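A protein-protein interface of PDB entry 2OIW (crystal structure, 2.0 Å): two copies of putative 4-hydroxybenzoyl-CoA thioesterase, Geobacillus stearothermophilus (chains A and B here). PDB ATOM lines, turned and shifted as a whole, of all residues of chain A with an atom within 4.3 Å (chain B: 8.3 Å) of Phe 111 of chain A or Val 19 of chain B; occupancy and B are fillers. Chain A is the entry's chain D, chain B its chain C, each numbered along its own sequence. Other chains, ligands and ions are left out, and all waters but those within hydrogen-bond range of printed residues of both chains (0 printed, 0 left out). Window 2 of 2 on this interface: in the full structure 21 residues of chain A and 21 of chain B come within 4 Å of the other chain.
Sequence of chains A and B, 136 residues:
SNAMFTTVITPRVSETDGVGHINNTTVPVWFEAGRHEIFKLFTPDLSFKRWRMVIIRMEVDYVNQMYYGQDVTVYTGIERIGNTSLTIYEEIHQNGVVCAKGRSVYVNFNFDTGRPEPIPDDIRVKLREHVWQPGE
No position is printed for both chains.
Of the 5 pairs that touch across the chains among the printed residues, none has its exchanged pair printed and touching as well.
Printed residues of chain B that touch a printed residue of chain A: Gly 18, Val 19 and Gln 65.
Of the 10 printed residues of chain A, 4 touch a printed residue of chain B.
Hydrophobic or aromatic side chains of chain A within 4 Å of the printed part of chain B: Phe 48, Trp 51, Val 54 and Phe 111.
Among the printed residues, 5 pairs touch across the chains.
Among the printed residues, no Asp or Glu carboxylate lies within 4 Å of a Lys or Arg side-chain nitrogen of the other chain.
Among the printed residues, pairs that only touch across the chains: Phe 48 of chain A with Gly 18 of chain B, Phe 48 of chain A with Val 19 of chain B, Trp 51 of chain A with Val 19 of chain B, Val 54 of chain A with Gln 65 of chain B and Phe 111 of chain A with Val 19 of chain B.
Of chain B, only Val 19 comes within 4 Å of Phe 111 of chain A.
Val 19 of chain B touches just these residues of chain A: Phe 48 (3.8 Å), Trp 51 (3.8 Å) and Phe 111 (3.5 Å).
Of the printed residues of chain B, Val 54 of chain A touches Gln 65 (3.6 Å).
Of the printed residues of chain B, Trp 51 of chain A touches Val 19 (3.8 Å).
Of the printed residues of chain B, Phe 48 of chain A touches Gly 18 (3.6 Å) and Val 19 (3.8 Å).
Printed residues of chain A within 4 Å of Gln 65 of chain B: Val 54 (3.6 Å).
Of the printed residues of chain A, Gly 18 of chain B touches Phe 48 (3.6 Å).
Gly 20 of chain B touches none of the printed residues of chain A.
Asn 23 of chain B touches none of the printed residues of chain A.
The nearest printed residue of chain A that does not touch Val 19 of chain B is Val 54 of chain A (5.8 Å).
A ring nitrogen (ND1) of His 21 of chain B lies close to the side-chain amide nitrogen (NE2) of Gln 65 of chain B (3.3 Å).
OD1 of Asp 17 of chain B sits at hydrogen-bond distance from N of Val 19 of chain B (3.1 Å).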
ATOM      1  N   PHE A  48      25.727  -1.126  -4.682  1.00  0.00           N
ATOM      2  CA  PHE A  48      25.430  -0.810  -3.278  1.00  0.00           C
ATOM      3  C   PHE A  48      24.402  -1.711  -2.596  1.00  0.00           C
ATOM      4  O   PHE A  48      24.438  -1.869  -1.378  1.00  0.00           O
ATOM      5  CB  PHE A  48      25.071   0.667  -3.070  1.00  0.00           C
ATOM      6  CG  PHE A  48      26.253   1.594  -3.183  1.00  0.00           C
ATOM      7  CD1 PHE A  48      27.249   1.586  -2.225  1.00  0.00           C
ATOM      8  CD2 PHE A  48      26.371   2.473  -4.255  1.00  0.00           C
ATOM      9  CE1 PHE A  48      28.343   2.432  -2.322  1.00  0.00           C
ATOM     10  CE2 PHE A  48      27.468   3.320  -4.350  1.00  0.00           C
ATOM     11  CZ  PHE A  48      28.449   3.285  -3.389  1.00  0.00           C
ATOM     12  N   TRP A  51      26.434  -4.356  -1.015  1.00  0.00           N
ATOM     13  CA  TRP A  51      27.557  -3.866  -0.218  1.00  0.00           C
ATOM     14  C   TRP A  51      27.665  -4.697   1.032  1.00  0.00           C
ATOM     15  O   TRP A  51      26.653  -5.196   1.542  1.00  0.00           O
ATOM     16  CB  TRP A  51      27.386  -2.399   0.150  1.00  0.00           C
ATOM     17  CG  TRP A  51      28.690  -1.717   0.396  1.00  0.00           C
ATOM     18  CD1 TRP A  51      29.240  -1.373   1.618  1.00  0.00           C
ATOM     19  CD2 TRP A  51      29.625  -1.284  -0.592  1.00  0.00           C
ATOM     20  NE1 TRP A  51      30.452  -0.763   1.434  1.00  0.00           N
ATOM     21  CE2 TRP A  51      30.723  -0.704   0.092  1.00  0.00           C
ATOM     22  CE3 TRP A  51      29.650  -1.334  -1.992  1.00  0.00           C
ATOM     23  CZ2 TRP A  51      31.814  -0.163  -0.576  1.00  0.00           C
ATOM     24  CZ3 TRP A  51      30.758  -0.805  -2.655  1.00  0.00           C
ATOM     25  CH2 TRP A  51      31.819  -0.230  -1.944  1.00  0.00           C
ATOM     26  N   ARG A  52      28.882  -4.856   1.529  1.00  0.00           N
ATOM     27  CA  ARG A  52      29.074  -5.614   2.756  1.00  0.00           C
ATOM     28  C   ARG A  52      30.244  -5.117   3.602  1.00  0.00           C
ATOM     29  O   ARG A  52      30.744  -5.859   4.425  1.00  0.00           O
ATOM     30  CB  ARG A  52      29.231  -7.126   2.451  1.00  0.00           C
ATOM     31  CG  ARG A  52      30.090  -7.462   1.244  1.00  0.00           C
ATOM     32  CD  ARG A  52      30.580  -8.916   1.254  1.00  0.00           C
ATOM     33  NE  ARG A  52      29.593  -9.896   0.802  1.00  0.00           N
ATOM     34  CZ  ARG A  52      29.417 -11.100   1.364  1.00  0.00           C
ATOM     35  NH1 ARG A  52      30.129 -11.466   2.431  1.00  0.00           N
ATOM     36  NH2 ARG A  52      28.501 -11.930   0.894  1.00  0.00           N
ATOM     37  N   VAL A  54      31.832  -2.329   6.277  1.00  0.00           N
ATOM     38  CA  VAL A  54      31.564  -1.255   7.209  1.00  0.00           C
ATOM     39  C   VAL A  54      32.854  -0.966   7.957  1.00  0.00           C
ATOM     40  O   VAL A  54      33.408  -1.876   8.576  1.00  0.00           O
ATOM     41  CB  VAL A  54      30.408  -1.643   8.173  1.00  0.00           C
ATOM     42  CG1 VAL A  54      30.407  -0.814   9.410  1.00  0.00           C
ATOM     43  CG2 VAL A  54      29.061  -1.516   7.451  1.00  0.00           C
ATOM     44  N   PHE A 109      29.799  -7.097   6.686  1.00  0.00           N
ATOM     45  CA  PHE A 109      28.541  -6.734   7.320  1.00  0.00           C
ATOM     46  C   PHE A 109      27.354  -7.165   6.475  1.00  0.00           C
ATOM     47  O   PHE A 109      27.349  -7.006   5.253  1.00  0.00           O
ATOM     48  CB  PHE A 109      28.478  -5.232   7.579  1.00  0.00           C
ATOM     49  CG  PHE A 109      27.397  -4.826   8.565  1.00  0.00           C
ATOM     50  CD1 PHE A 109      27.647  -4.830   9.930  1.00  0.00           C
ATOM     51  CD2 PHE A 109      26.140  -4.392   8.109  1.00  0.00           C
ATOM     52  CE1 PHE A 109      26.635  -4.422  10.850  1.00  0.00           C
ATOM     53  CE2 PHE A 109      25.126  -3.980   9.003  1.00  0.00           C
ATOM     54  CZ  PHE A 109      25.365  -4.007  10.367  1.00  0.00           C
ATOM     55  N   ASN A 110      26.351  -7.724   7.140  1.00  0.00           N
ATOM     56  CA  ASN A 110      25.151  -8.173   6.480  1.00  0.00           C
ATOM     57  C   ASN A 110      24.062  -7.165   6.788  1.00  0.00           C
ATOM     58  O   ASN A 110      23.518  -7.161   7.889  1.00  0.00           O
ATOM     59  CB  ASN A 110      24.759  -9.546   7.032  1.00  0.00           C
ATOM     60  CG  ASN A 110      23.600 -10.170   6.280  1.00  0.00           C
ATOM     61  OD1 ASN A 110      22.763  -9.482   5.715  1.00  0.00           O
ATOM     62  ND2 ASN A 110      23.557 -11.486   6.272  1.00  0.00           N
ATOM     63  N   PHE A 111      23.773  -6.305   5.815  1.00  0.00           N
ATOM     64  CA  PHE A 111      22.731  -5.280   5.950  1.00  0.00           C
ATOM     65  C   PHE A 111      21.315  -5.864   5.954  1.00  0.00           C
ATOM     66  O   PHE A 111      20.375  -5.168   6.318  1.00  0.00           O
ATOM     67  CB  PHE A 111      22.873  -4.179   4.865  1.00  0.00           C
ATOM     68  CG  PHE A 111      24.090  -3.323   5.042  1.00  0.00           C
ATOM     69  CD1 PHE A 111      24.087  -2.280   5.969  1.00  0.00           C
ATOM     70  CD2 PHE A 111      25.259  -3.579   4.315  1.00  0.00           C
ATOM     71  CE1 PHE A 111      25.220  -1.490   6.171  1.00  0.00           C
ATOM     72  CE2 PHE A 111      26.415  -2.793   4.509  1.00  0.00           C
ATOM     73  CZ  PHE A 111      26.384  -1.743   5.439  1.00  0.00           C
ATOM     74  N   ASP A 112      21.166  -7.140   5.571  1.00  0.00           N
ATOM     75  CA  ASP A 112      19.849  -7.819   5.624  1.00  0.00           C
ATOM     76  C   ASP A 112      19.471  -8.189   7.044  1.00  0.00           C
ATOM     77  O   ASP A 112      18.308  -8.082   7.402  1.00  0.00           O
ATOM     78  CB  ASP A 112      19.829  -9.096   4.767  1.00  0.00           C
ATOM     79  CG  ASP A 112      20.230  -8.840   3.311  1.00  0.00           C
ATOM     80  OD1 ASP A 112      19.560  -8.013   2.645  1.00  0.00           O
ATOM     81  OD2 ASP A 112      21.197  -9.489   2.834  1.00  0.00           O
ATOM     82  N   THR A 113      20.451  -8.637   7.839  1.00  0.00           N
ATOM     83  CA  THR A 113      20.216  -9.068   9.223  1.00  0.00           C
ATOM     84  C   THR A 113      20.697  -8.025  10.220  1.00  0.00           C
ATOM     85  O   THR A 113      20.428  -8.141  11.406  1.00  0.00           O
ATOM     86  CB  THR A 113      20.960 -10.379   9.554  1.00  0.00           C
ATOM     87  OG1 THR A 113      22.354 -10.166   9.348  1.00  0.00           O
ATOM     88  CG2 THR A 113      20.497 -11.556   8.646  1.00  0.00           C
ATOM     89  N   GLY A 114      21.452  -7.042   9.742  1.00  0.00           N
ATOM     90  CA  GLY A 114      21.971  -5.974  10.595  1.00  0.00           C
ATOM     91  C   GLY A 114      23.099  -6.388  11.549  1.00  0.00           C
ATOM     92  O   GLY A 114      23.280  -5.781  12.593  1.00  0.00           O
ATOM     93  N   THR B  16      26.373  11.670   2.764  1.00  0.00           N
ATOM     94  CA  THR B  16      26.069  10.244   2.820  1.00  0.00           C
ATOM     95  C   THR B  16      26.851   9.560   1.693  1.00  0.00           C
ATOM     96  O   THR B  16      27.594  10.230   0.970  1.00  0.00           O
ATOM     97  CB  THR B  16      24.547   9.988   2.684  1.00  0.00           C
ATOM     98  OG1 THR B  16      24.061  10.557   1.449  1.00  0.00           O
ATOM     99  CG2 THR B  16      23.820  10.625   3.864  1.00  0.00           C
ATOM    100  N   ASP B  17      26.743   8.238   1.585  1.00  0.00           N
ATOM    101  CA  ASP B  17      27.191   7.529   0.383  1.00  0.00           C
ATOM    102  C   ASP B  17      26.089   6.547   0.002  1.00  0.00           C
ATOM    103  O   ASP B  17      25.083   6.487   0.682  1.00  0.00           O
ATOM    104  CB  ASP B  17      28.502   6.796   0.610  1.00  0.00           C
ATOM    105  CG  ASP B  17      28.446   5.841   1.803  1.00  0.00           C
ATOM    106  OD1 ASP B  17      27.327   5.366   2.164  1.00  0.00           O
ATOM    107  OD2 ASP B  17      29.534   5.574   2.392  1.00  0.00           O
ATOM    108  N   GLY B  18      26.305   5.751  -1.041  1.00  0.00           N
ATOM    109  CA  GLY B  18      25.282   4.842  -1.543  1.00  0.00           C
ATOM    110  C   GLY B  18      24.762   3.790  -0.565  1.00  0.00           C
ATOM    111  O   GLY B  18      23.729   3.188  -0.815  1.00  0.00           O
ATOM    112  N   VAL B  19      25.479   3.550   0.536  1.00  0.00           N
ATOM    113  CA  VAL B  19      25.050   2.552   1.524  1.00  0.00           C
ATOM    114  C   VAL B  19      23.829   3.102   2.271  1.00  0.00           C
ATOM    115  O   VAL B  19      22.999   2.336   2.832  1.00  0.00           O
ATOM    116  CB  VAL B  19      26.173   2.171   2.527  1.00  0.00           C
ATOM    117  CG1 VAL B  19      25.848   0.844   3.183  1.00  0.00           C
ATOM    118  CG2 VAL B  19      27.546   2.074   1.832  1.00  0.00           C
ATOM    119  N   GLY B  20      23.710   4.430   2.262  1.00  0.00           N
ATOM    120  CA  GLY B  20      22.530   5.083   2.827  1.00  0.00           C
ATOM    121  C   GLY B  20      22.762   5.816   4.115  1.00  0.00           C
ATOM    122  O   GLY B  20      21.849   6.464   4.646  1.00  0.00           O
ATOM    123  N   HIS B  21      23.971   5.687   4.646  1.00  0.00           N
ATOM    124  CA  HIS B  21      24.339   6.376   5.855  1.00  0.00           C
ATOM    125  C   HIS B  21      25.428   7.421   5.565  1.00  0.00           C
ATOM    126  O   HIS B  21      25.939   7.499   4.437  1.00  0.00           O
ATOM    127  CB  HIS B  21      24.810   5.359   6.908  1.00  0.00           C
ATOM    128  CG  HIS B  21      25.940   4.479   6.449  1.00  0.00           C
ATOM    129  ND1 HIS B  21      25.980   3.128   6.719  1.00  0.00           N
ATOM    130  CD2 HIS B  21      27.080   4.758   5.767  1.00  0.00           C
ATOM    131  CE1 HIS B  21      27.095   2.612   6.223  1.00  0.00           C
ATOM    132  NE2 HIS B  21      27.776   3.578   5.634  1.00  0.00           N
ATOM    133  N   ILE B  22      25.790   8.195   6.590  1.00  0.00           N
ATOM    134  CA  ILE B  22      26.887   9.164   6.507  1.00  0.00           C
ATOM    135  C   ILE B  22      28.176   8.420   6.183  1.00  0.00           C
ATOM    136  O   ILE B  22      28.469   7.391   6.800  1.00  0.00           O
ATOM    137  CB  ILE B  22      27.054   9.915   7.832  1.00  0.00           C
ATOM    138  CG1 ILE B  22      25.801  10.742   8.139  1.00  0.00           C
ATOM    139  CG2 ILE B  22      28.301  10.807   7.817  1.00  0.00           C
ATOM    140  CD1 ILE B  22      25.522  11.907   7.166  1.00  0.00           C
ATOM    141  N   ASN B  23      28.933   8.934   5.211  1.00  0.00           N
ATOM    142  CA  ASN B  23      30.196   8.308   4.794  1.00  0.00           C
ATOM    143  C   ASN B  23      31.256   8.553   5.854  1.00  0.00           C
ATOM    144  O   ASN B  23      31.280   9.613   6.495  1.00  0.00           O
ATOM    145  CB  ASN B  23      30.653   8.884   3.440  1.00  0.00           C
ATOM    146  CG  ASN B  23      31.950   8.283   2.936  1.00  0.00           C
ATOM    147  OD1 ASN B  23      33.016   8.901   3.058  1.00  0.00           O
ATOM    148  ND2 ASN B  23      31.877   7.083   2.361  1.00  0.00           N
ATOM    149  N   ASN B  24      32.119   7.558   6.054  1.00  0.00           N
ATOM    150  CA  ASN B  24      33.180   7.647   7.043  1.00  0.00           C
ATOM    151  C   ASN B  24      34.075   8.867   6.864  1.00  0.00           C
ATOM    152  O   ASN B  24      34.609   9.395   7.859  1.00  0.00           O
ATOM    153  CB  ASN B  24      34.014   6.376   7.032  1.00  0.00           C
ATOM    154  CG  ASN B  24      34.825   6.226   5.768  1.00  0.00           C
ATOM    155  OD1 ASN B  24      35.986   6.624   5.703  1.00  0.00           O
ATOM    156  ND2 ASN B  24      34.222   5.654   4.758  1.00  0.00           N
ATOM    157  N   GLN B  65      26.330   3.860  13.199  1.00  0.00           N
ATOM    158  CA  GLN B  65      26.096   4.575  11.929  1.00  0.00           C
ATOM    159  C   GLN B  65      25.271   5.834  12.167  1.00  0.00           C
ATOM    160  O   GLN B  65      24.422   5.869  13.055  1.00  0.00           O
ATOM    161  CB  GLN B  65      25.377   3.699  10.905  1.00  0.00           C
ATOM    162  CG  GLN B  65      26.089   2.401  10.548  1.00  0.00           C
ATOM    163  CD  GLN B  65      27.284   2.587   9.611  1.00  0.00           C
ATOM    164  OE1 GLN B  65      27.803   3.704   9.423  1.00  0.00           O
ATOM    165  NE2 GLN B  65      27.718   1.485   8.996  1.00  0.00           N
ATOM    166  N   TYR B  67      22.926   9.096  10.267  1.00  0.00           N
ATOM    167  CA  TYR B  67      22.038   9.265   9.145  1.00  0.00           C
ATOM    168  C   TYR B  67      21.802  10.739   8.849  1.00  0.00           C
ATOM    169  O   TYR B  67      21.867  11.589   9.747  1.00  0.00           O
ATOM    170  CB  TYR B  67      20.717   8.486   9.398  1.00  0.00           C
ATOM    171  CG  TYR B  67      21.000   6.996   9.430  1.00  0.00           C
ATOM    172  CD1 TYR B  67      21.199   6.291   8.242  1.00  0.00           C
ATOM    173  CD2 TYR B  67      21.186   6.322  10.647  1.00  0.00           C
ATOM    174  CE1 TYR B  67      21.533   4.933   8.255  1.00  0.00           C
ATOM    175  CE2 TYR B  67      21.524   4.972  10.680  1.00  0.00           C
ATOM    176  CZ  TYR B  67      21.697   4.279   9.471  1.00  0.00           C
ATOM    177  OH  TYR B  67      22.023   2.935   9.474  1.00  0.00           O
